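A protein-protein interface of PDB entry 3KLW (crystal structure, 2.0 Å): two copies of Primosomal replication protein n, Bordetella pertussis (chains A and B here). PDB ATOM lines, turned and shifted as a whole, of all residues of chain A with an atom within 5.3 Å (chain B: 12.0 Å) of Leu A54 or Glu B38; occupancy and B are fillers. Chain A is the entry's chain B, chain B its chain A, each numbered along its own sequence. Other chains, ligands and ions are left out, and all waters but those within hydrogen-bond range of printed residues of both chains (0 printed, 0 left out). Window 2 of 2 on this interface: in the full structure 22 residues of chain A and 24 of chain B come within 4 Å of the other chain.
Leu A23 touches Ala B39 (CD2 to CB, 3.3 Å).
Leu A54 touches Glu B38 (CD2 to OE2, 3.8 Å).
Leu A54 touches Ala B39 (CD2 to CB, 3.5 Å).
Val B36 touches Phe A75.
Phe A75 touches Glu B38.
Phe A75 touches Arg B43 (CE1 to NH1, 3.8 Å).
Phe A75 touches Val B45 (CE1 to CG2, 3.7 Å).
No position is printed for both chains.
Of the 8 pairs that touch across the chains among the printed residues, none has its exchanged pair printed and touching as well.
Of the 13 printed residues of chain B, 5 touch a printed residue of chain A.
Hydrophobic or aromatic side chains of chain B that line the printed part of chain A: Val B36, Ala B39 and Val B45.
Along chain B the printed residues that touch a printed residue of chain A span positions 36 to 45.
Hydrophobic or aromatic side chains of chain A within 4 Å of the printed part of chain B: Leu A23, Leu A54, Phe A75 and His A89.
Along chain A the printed residues that touch a printed residue of chain B span positions 23 to 89.
Among the printed residues, no Asp or Glu carboxylate lies within 4 Å of a Lys or Arg side-chain nitrogen of the other chain.
A ring nitrogen (ND1) of His A89 sits at hydrogen-bond distance from the side-chain carboxylate (OE2) of Glu B38 (2.8 Å).
The backbone NH (N) of Val B45 lies within hydrogen-bond range of the backbone carbonyl oxygen (O) of Ser B34 (2.7 Å).
The side-chain carboxylate (OE1) of Glu B38 lies within salt-bridge range of the guanidinium group (NE) of Arg B43, 3.6 Å away.
The backbone carbonyl oxygen of Ala B39 sits close to a ring nitrogen (NE2) of His B41 (3.4 Å).
The backbone NH (N) of Leu A23 sits close to the side-chain hydroxyl (OG1) of Thr A19, 3.4 Å away.
The backbone carbonyl oxygen (O) of Phe A75 sits at hydrogen-bond distance from the backbone NH (N) of His A89.
The backbone NH (N) of Arg B43 lies within hydrogen-bond range of the backbone carbonyl oxygen (O) of Val B36, 2.7 Å away.
Leu A23 touches one residue of chain B.
No residue of chain B comes within 4 Å of Pro A24.
No residue of chain B comes within 4 Å of Ala A25.
No residue of chain B comes within 4 Å of Val A52.
No residue of chain B comes within 4 Å of Ala A53.
Leu A54 touches just these residues of chain B: Glu B38 and Ala B39.
No residue of chain B comes within 4 Å of Asp A56.
No residue of chain B comes within 4 Å of Leu A57.
No residue of chain B comes within 4 Å of Ala A58.
Ser B34 touches none of the printed residues of chain A.
Glu B38 touches three residues of chain A.
Printed residues of chain A within 4 Å of Arg B43: Phe A75.
Printed residues of chain A within 4 Å of Val B45: Phe A75 (3.7 Å).
The nearest residue of chain B that does not touch Leu A54 is His B41 (6.0 Å).
The nearest residue of chain A that does not touch Glu B38 is Val A52 (4.5 Å).
The nearest printed residue of chain B that does not touch Phe A75 is Val B37 (4.7 Å).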
ATOM      1  N   THR A  19      16.333   3.272   6.075  1.00  0.00           N
ATOM      2  CA  THR A  19      16.071   4.592   5.497  1.00  0.00           C
ATOM      3  C   THR A  19      17.373   5.106   4.838  1.00  0.00           C
ATOM      4  O   THR A  19      18.442   4.517   5.017  1.00  0.00           O
ATOM      5  CB  THR A  19      15.658   5.589   6.588  1.00  0.00           C
ATOM      6  OG1 THR A  19      16.736   5.750   7.521  1.00  0.00           O
ATOM      7  CG2 THR A  19      14.424   5.085   7.344  1.00  0.00           C
ATOM      8  N   LEU A  23      19.214   3.944   8.931  1.00  0.00           N
ATOM      9  CA  LEU A  23      18.454   3.570  10.119  1.00  0.00           C
ATOM     10  C   LEU A  23      17.527   2.391   9.820  1.00  0.00           C
ATOM     11  O   LEU A  23      16.842   2.404   8.811  1.00  0.00           O
ATOM     12  CB  LEU A  23      17.629   4.763  10.575  1.00  0.00           C
ATOM     13  CG  LEU A  23      17.254   4.750  12.034  1.00  0.00           C
ATOM     14  CD1 LEU A  23      18.528   4.669  12.900  1.00  0.00           C
ATOM     15  CD2 LEU A  23      16.466   6.044  12.329  1.00  0.00           C
ATOM     16  N   PRO A  24      17.527   1.348  10.677  1.00  0.00           N
ATOM     17  CA  PRO A  24      16.673   0.161  10.512  1.00  0.00           C
ATOM     18  C   PRO A  24      15.205   0.609  10.559  1.00  0.00           C
ATOM     19  O   PRO A  24      14.841   1.385  11.438  1.00  0.00           O
ATOM     20  CB  PRO A  24      17.003  -0.696  11.730  1.00  0.00           C
ATOM     21  CG  PRO A  24      18.363  -0.266  12.132  1.00  0.00           C
ATOM     22  CD  PRO A  24      18.454   1.194  11.809  1.00  0.00           C
ATOM     23  N   ALA A  25      14.379   0.131   9.630  1.00  0.00           N
ATOM     24  CA  ALA A  25      12.948   0.503   9.567  1.00  0.00           C
ATOM     25  C   ALA A  25      12.074  -0.722   9.280  1.00  0.00           C
ATOM     26  O   ALA A  25      12.406  -1.547   8.411  1.00  0.00           O
ATOM     27  CB  ALA A  25      12.735   1.548   8.485  1.00  0.00           C
ATOM     28  N   LEU A  26      10.958  -0.828   9.997  1.00  0.00           N
ATOM     29  CA  LEU A  26      10.047  -1.958   9.866  1.00  0.00           C
ATOM     30  C   LEU A  26       8.579  -1.501   9.842  1.00  0.00           C
ATOM     31  O   LEU A  26       8.203  -0.596  10.594  1.00  0.00           O
ATOM     32  CB  LEU A  26      10.227  -2.898  11.066  1.00  0.00           C
ATOM     33  CG  LEU A  26       9.379  -4.190  11.027  1.00  0.00           C
ATOM     34  CD1 LEU A  26      10.061  -5.201  10.067  1.00  0.00           C
ATOM     35  CD2 LEU A  26       9.279  -4.833  12.408  1.00  0.00           C
ATOM     36  N   VAL A  52       4.701   1.726  12.452  1.00  0.00           N
ATOM     37  CA  VAL A  52       6.055   1.833  11.913  1.00  0.00           C
ATOM     38  C   VAL A  52       7.052   1.885  13.067  1.00  0.00           C
ATOM     39  O   VAL A  52       6.855   2.651  14.013  1.00  0.00           O
ATOM     40  CB  VAL A  52       6.276   3.110  11.004  1.00  0.00           C
ATOM     41  CG1 VAL A  52       5.552   2.957   9.657  1.00  0.00           C
ATOM     42  CG2 VAL A  52       5.784   4.326  11.665  1.00  0.00           C
ATOM     43  N   ALA A  53       8.087   1.039  13.000  1.00  0.00           N
ATOM     44  CA  ALA A  53       9.152   0.969  14.009  1.00  0.00           C
ATOM     45  C   ALA A  53      10.500   1.391  13.382  1.00  0.00           C
ATOM     46  O   ALA A  53      10.852   0.969  12.279  1.00  0.00           O
ATOM     47  CB  ALA A  53       9.275  -0.467  14.587  1.00  0.00           C
ATOM     48  N   LEU A  54      11.234   2.220  14.116  1.00  0.00           N
ATOM     49  CA  LEU A  54      12.541   2.719  13.724  1.00  0.00           C
ATOM     50  C   LEU A  54      13.672   2.311  14.709  1.00  0.00           C
ATOM     51  O   LEU A  54      13.435   1.998  15.901  1.00  0.00           O
ATOM     52  CB  LEU A  54      12.470   4.236  13.636  1.00  0.00           C
ATOM     53  CG  LEU A  54      12.775   4.922  12.304  1.00  0.00           C
ATOM     54  CD1 LEU A  54      11.940   4.371  11.163  1.00  0.00           C
ATOM     55  CD2 LEU A  54      12.509   6.403  12.486  1.00  0.00           C
ATOM     56  N   GLY A  55      14.903   2.297  14.189  1.00  0.00           N
ATOM     57  CA  GLY A  55      16.067   1.988  14.996  1.00  0.00           C
ATOM     58  C   GLY A  55      15.979   0.710  15.778  1.00  0.00           C
ATOM     59  O   GLY A  55      15.662  -0.324  15.232  1.00  0.00           O
ATOM     60  N   ASP A  56      16.250   0.798  17.072  1.00  0.00           N
ATOM     61  CA  ASP A  56      16.228  -0.347  17.983  1.00  0.00           C
ATOM     62  C   ASP A  56      14.885  -1.125  18.041  1.00  0.00           C
ATOM     63  O   ASP A  56      14.858  -2.365  18.153  1.00  0.00           O
ATOM     64  CB  ASP A  56      16.623   0.160  19.371  1.00  0.00           C
ATOM     65  CG  ASP A  56      17.604  -0.748  20.074  1.00  0.00           C
ATOM     66  OD1 ASP A  56      18.792  -0.822  19.649  1.00  0.00           O
ATOM     67  OD2 ASP A  56      17.176  -1.386  21.067  1.00  0.00           O
ATOM     68  N   LEU A  57      13.765  -0.405  17.972  1.00  0.00           N
ATOM     69  CA  LEU A  57      12.465  -1.064  18.000  1.00  0.00           C
ATOM     70  C   LEU A  57      12.223  -1.956  16.787  1.00  0.00           C
ATOM     71  O   LEU A  57      11.583  -2.984  16.890  1.00  0.00           O
ATOM     72  CB  LEU A  57      11.359  -0.021  18.107  1.00  0.00           C
ATOM     73  CG  LEU A  57      11.224   0.613  19.480  1.00  0.00           C
ATOM     74  CD1 LEU A  57       9.968   1.510  19.529  1.00  0.00           C
ATOM     75  CD2 LEU A  57      11.100  -0.496  20.509  1.00  0.00           C
ATOM     76  N   ALA A  58      12.705  -1.520  15.630  1.00  0.00           N
ATOM     77  CA  ALA A  58      12.616  -2.315  14.409  1.00  0.00           C
ATOM     78  C   ALA A  58      13.378  -3.657  14.602  1.00  0.00           C
ATOM     79  O   ALA A  58      12.896  -4.737  14.167  1.00  0.00           O
ATOM     80  CB  ALA A  58      13.238  -1.539  13.255  1.00  0.00           C
ATOM     81  N   PHE A  75       3.150   7.698  18.758  1.00  0.00           N
ATOM     82  CA  PHE A  75       2.304   8.779  18.297  1.00  0.00           C
ATOM     83  C   PHE A  75       1.689   8.459  16.900  1.00  0.00           C
ATOM     84  O   PHE A  75       2.258   7.664  16.100  1.00  0.00           O
ATOM     85  CB  PHE A  75       3.098  10.091  18.250  1.00  0.00           C
ATOM     86  CG  PHE A  75       4.239  10.081  17.240  1.00  0.00           C
ATOM     87  CD1 PHE A  75       4.019  10.425  15.927  1.00  0.00           C
ATOM     88  CD2 PHE A  75       5.543   9.741  17.636  1.00  0.00           C
ATOM     89  CE1 PHE A  75       5.091  10.412  14.978  1.00  0.00           C
ATOM     90  CE2 PHE A  75       6.604   9.724  16.719  1.00  0.00           C
ATOM     91  CZ  PHE A  75       6.377  10.071  15.387  1.00  0.00           C
ATOM     92  N   HIS A  89       3.452   5.485  14.904  1.00  0.00           N
ATOM     93  CA  HIS A  89       4.922   5.571  14.976  1.00  0.00           C
ATOM     94  C   HIS A  89       5.321   5.094  16.369  1.00  0.00           C
ATOM     95  O   HIS A  89       5.179   5.823  17.368  1.00  0.00           O
ATOM     96  CB  HIS A  89       5.365   7.004  14.745  1.00  0.00           C
ATOM     97  CG  HIS A  89       5.186   7.420  13.328  1.00  0.00           C
ATOM     98  ND1 HIS A  89       6.226   7.408  12.424  1.00  0.00           N
ATOM     99  CD2 HIS A  89       4.067   7.671  12.610  1.00  0.00           C
ATOM    100  CE1 HIS A  89       5.753   7.631  11.209  1.00  0.00           C
ATOM    101  NE2 HIS A  89       4.447   7.792  11.294  1.00  0.00           N
ATOM    102  N   LEU A  90       5.777   3.849  16.433  1.00  0.00           N
ATOM    103  CA  LEU A  90       6.135   3.209  17.694  1.00  0.00           C
ATOM    104  C   LEU A  90       7.275   3.873  18.456  1.00  0.00           C
ATOM    105  O   LEU A  90       8.310   4.240  17.878  1.00  0.00           O
ATOM    106  CB  LEU A  90       6.505   1.723  17.445  1.00  0.00           C
ATOM    107  CG  LEU A  90       5.419   0.879  16.737  1.00  0.00           C
ATOM    108  CD1 LEU A  90       5.913  -0.570  16.444  1.00  0.00           C
ATOM    109  CD2 LEU A  90       4.180   0.825  17.604  1.00  0.00           C
ATOM    110  N   SER B  34       2.333  19.267  16.365  1.00  0.00           N
ATOM    111  CA  SER B  34       3.412  19.242  17.349  1.00  0.00           C
ATOM    112  C   SER B  34       4.681  18.705  16.753  1.00  0.00           C
ATOM    113  O   SER B  34       4.706  18.207  15.604  1.00  0.00           O
ATOM    114  CB  SER B  34       3.054  18.387  18.581  1.00  0.00           C
ATOM    115  OG  SER B  34       3.121  16.997  18.323  1.00  0.00           O
ATOM    116  N   GLU B  35       5.753  18.821  17.532  1.00  0.00           N
ATOM    117  CA  GLU B  35       7.049  18.313  17.100  1.00  0.00           C
ATOM    118  C   GLU B  35       7.362  17.125  17.996  1.00  0.00           C
ATOM    119  O   GLU B  35       7.139  17.173  19.209  1.00  0.00           O
ATOM    120  CB  GLU B  35       8.144  19.380  17.254  1.00  0.00           C
ATOM    121  CG  GLU B  35       8.061  20.523  16.241  1.00  0.00           C
ATOM    122  CD  GLU B  35       8.672  20.181  14.894  1.00  0.00           C
ATOM    123  OE1 GLU B  35       9.884  19.835  14.843  1.00  0.00           O
ATOM    124  OE2 GLU B  35       7.945  20.271  13.875  1.00  0.00           O
ATOM    125  N   VAL B  36       7.837  16.050  17.392  1.00  0.00           N
ATOM    126  CA  VAL B  36       8.213  14.863  18.152  1.00  0.00           C
ATOM    127  C   VAL B  36       9.588  14.359  17.681  1.00  0.00           C
ATOM    128  O   VAL B  36      10.025  14.619  16.556  1.00  0.00           O
ATOM    129  CB  VAL B  36       7.199  13.701  17.979  1.00  0.00           C
ATOM    130  CG1 VAL B  36       5.850  14.088  18.567  1.00  0.00           C
ATOM    131  CG2 VAL B  36       7.070  13.345  16.515  1.00  0.00           C
ATOM    132  N   VAL B  37      10.268  13.640  18.555  1.00  0.00           N
ATOM    133  CA  VAL B  37      11.567  13.073  18.226  1.00  0.00           C
ATOM    134  C   VAL B  37      11.354  11.589  17.871  1.00  0.00           C
ATOM    135  O   VAL B  37      10.707  10.860  18.632  1.00  0.00           O
ATOM    136  CB  VAL B  37      12.491  13.200  19.435  1.00  0.00           C
ATOM    137  CG1 VAL B  37      11.868  12.485  20.607  1.00  0.00           C
ATOM    138  CG2 VAL B  37      13.861  12.657  19.107  1.00  0.00           C
ATOM    139  N   GLU B  38      11.869  11.148  16.713  1.00  0.00           N
ATOM    140  CA  GLU B  38      11.725   9.740  16.277  1.00  0.00           C
ATOM    141  C   GLU B  38      13.105   9.130  15.965  1.00  0.00           C
ATOM    142  O   GLU B  38      13.831   9.643  15.110  1.00  0.00           O
ATOM    143  CB  GLU B  38      10.840   9.639  15.023  1.00  0.00           C
ATOM    144  CG  GLU B  38       9.781   8.541  15.077  1.00  0.00           C
ATOM    145  CD  GLU B  38       9.211   8.228  13.712  1.00  0.00           C
ATOM    146  OE1 GLU B  38       9.129   9.159  12.877  1.00  0.00           O
ATOM    147  OE2 GLU B  38       8.850   7.051  13.469  1.00  0.00           O
ATOM    148  N   ALA B  39      13.450   8.040  16.657  1.00  0.00           N
ATOM    149  CA  ALA B  39      14.743   7.377  16.488  1.00  0.00           C
ATOM    150  C   ALA B  39      15.893   8.375  16.685  1.00  0.00           C
ATOM    151  O   ALA B  39      16.969   8.214  16.103  1.00  0.00           O
ATOM    152  CB  ALA B  39      14.832   6.749  15.112  1.00  0.00           C
ATOM    153  N   GLY B  40      15.652   9.408  17.497  1.00  0.00           N
ATOM    154  CA  GLY B  40      16.659  10.421  17.764  1.00  0.00           C
ATOM    155  C   GLY B  40      16.716  11.561  16.762  1.00  0.00           C
ATOM    156  O   GLY B  40      17.777  12.148  16.588  1.00  0.00           O
ATOM    157  N   HIS B  41      15.592  11.879  16.112  1.00  0.00           N
ATOM    158  CA  HIS B  41      15.503  12.972  15.120  1.00  0.00           C
ATOM    159  C   HIS B  41      14.190  13.785  15.230  1.00  0.00           C
ATOM    160  O   HIS B  41      13.126  13.220  15.441  1.00  0.00           O
ATOM    161  CB  HIS B  41      15.593  12.393  13.705  1.00  0.00           C
ATOM    162  CG  HIS B  41      16.793  11.531  13.489  1.00  0.00           C
ATOM    163  ND1 HIS B  41      17.997  12.032  13.041  1.00  0.00           N
ATOM    164  CD2 HIS B  41      16.999  10.216  13.741  1.00  0.00           C
ATOM    165  CE1 HIS B  41      18.896  11.062  13.028  1.00  0.00           C
ATOM    166  NE2 HIS B  41      18.317   9.951  13.451  1.00  0.00           N
ATOM    167  N   PRO B  42      14.254  15.118  15.065  1.00  0.00           N
ATOM    168  CA  PRO B  42      13.048  15.956  15.153  1.00  0.00           C
ATOM    169  C   PRO B  42      12.076  15.692  14.001  1.00  0.00           C
ATOM    170  O   PRO B  42      12.502  15.377  12.895  1.00  0.00           O
ATOM    171  CB  PRO B  42      13.610  17.371  15.122  1.00  0.00           C
ATOM    172  CG  PRO B  42      14.822  17.218  14.247  1.00  0.00           C
ATOM    173  CD  PRO B  42      15.443  15.936  14.762  1.00  0.00           C
ATOM    174  N   ARG B  43      10.778  15.836  14.252  1.00  0.00           N
ATOM    175  CA  ARG B  43       9.771  15.581  13.216  1.00  0.00           C
ATOM    176  C   ARG B  43       8.462  16.336  13.475  1.00  0.00           C
ATOM    177  O   ARG B  43       7.904  16.298  14.570  1.00  0.00           O
ATOM    178  CB  ARG B  43       9.484  14.078  13.130  1.00  0.00           C
ATOM    179  CG  ARG B  43       8.525  13.668  12.023  1.00  0.00           C
ATOM    180  CD  ARG B  43       8.234  12.166  12.074  1.00  0.00           C
ATOM    181  NE  ARG B  43       7.418  11.695  10.953  1.00  0.00           N
ATOM    182  CZ  ARG B  43       6.096  11.844  10.848  1.00  0.00           C
ATOM    183  NH1 ARG B  43       5.408  12.461  11.802  1.00  0.00           N
ATOM    184  NH2 ARG B  43       5.456  11.373   9.782  1.00  0.00           N
ATOM    185  N   ARG B  44       7.982  17.017  12.449  1.00  0.00           N
ATOM    186  CA  ARG B  44       6.756  17.771  12.549  1.00  0.00           C
ATOM    187  C   ARG B  44       5.602  16.778  12.397  1.00  0.00           C
ATOM    188  O   ARG B  44       5.642  15.897  11.536  1.00  0.00           O
ATOM    189  CB  ARG B  44       6.706  18.802  11.423  1.00  0.00           C
ATOM    190  CG  ARG B  44       8.093  19.224  10.902  1.00  0.00           C
ATOM    191  CD  ARG B  44       7.982  20.187   9.722  1.00  0.00           C
ATOM    192  NE  ARG B  44       7.055  21.272  10.028  1.00  0.00           N
ATOM    193  CZ  ARG B  44       6.703  22.235   9.178  1.00  0.00           C
ATOM    194  NH1 ARG B  44       5.848  23.172   9.571  1.00  0.00           N
ATOM    195  NH2 ARG B  44       7.194  22.267   7.942  1.00  0.00           N
ATOM    196  N   VAL B  45       4.594  16.870  13.252  1.00  0.00           N
ATOM    197  CA  VAL B  45       3.447  15.983  13.103  1.00  0.00           C
ATOM    198  C   VAL B  45       2.189  16.839  13.039  1.00  0.00           C
ATOM    199  O   VAL B  45       1.952  17.639  13.936  1.00  0.00           O
ATOM    200  CB  VAL B  45       3.286  14.996  14.286  1.00  0.00           C
ATOM    201  CG1 VAL B  45       1.941  14.269  14.167  1.00  0.00           C
ATOM    202  CG2 VAL B  45       4.422  13.979  14.305  1.00  0.00           C
ATOM    203  N   GLU B  46       1.417  16.706  11.965  1.00  0.00           N
ATOM    204  CA  GLU B  46       0.146  17.422  11.824  1.00  0.00           C
ATOM    205  C   GLU B  46      -0.876  16.323  11.486  1.00  0.00           C
ATOM    206  O   GLU B  46      -0.798  15.709  10.435  1.00  0.00           O
ATOM    207  CB  GLU B  46       0.211  18.466  10.707  1.00  0.00           C
ATOM    208  CG  GLU B  46      -1.119  19.153  10.417  1.00  0.00           C
ATOM    209  CD  GLU B  46      -0.947  20.580   9.867  1.00  0.00           C
ATOM    210  OE1 GLU B  46      -0.204  20.759   8.863  1.00  0.00           O
ATOM    211  OE2 GLU B  46      -1.561  21.517  10.448  1.00  0.00           O
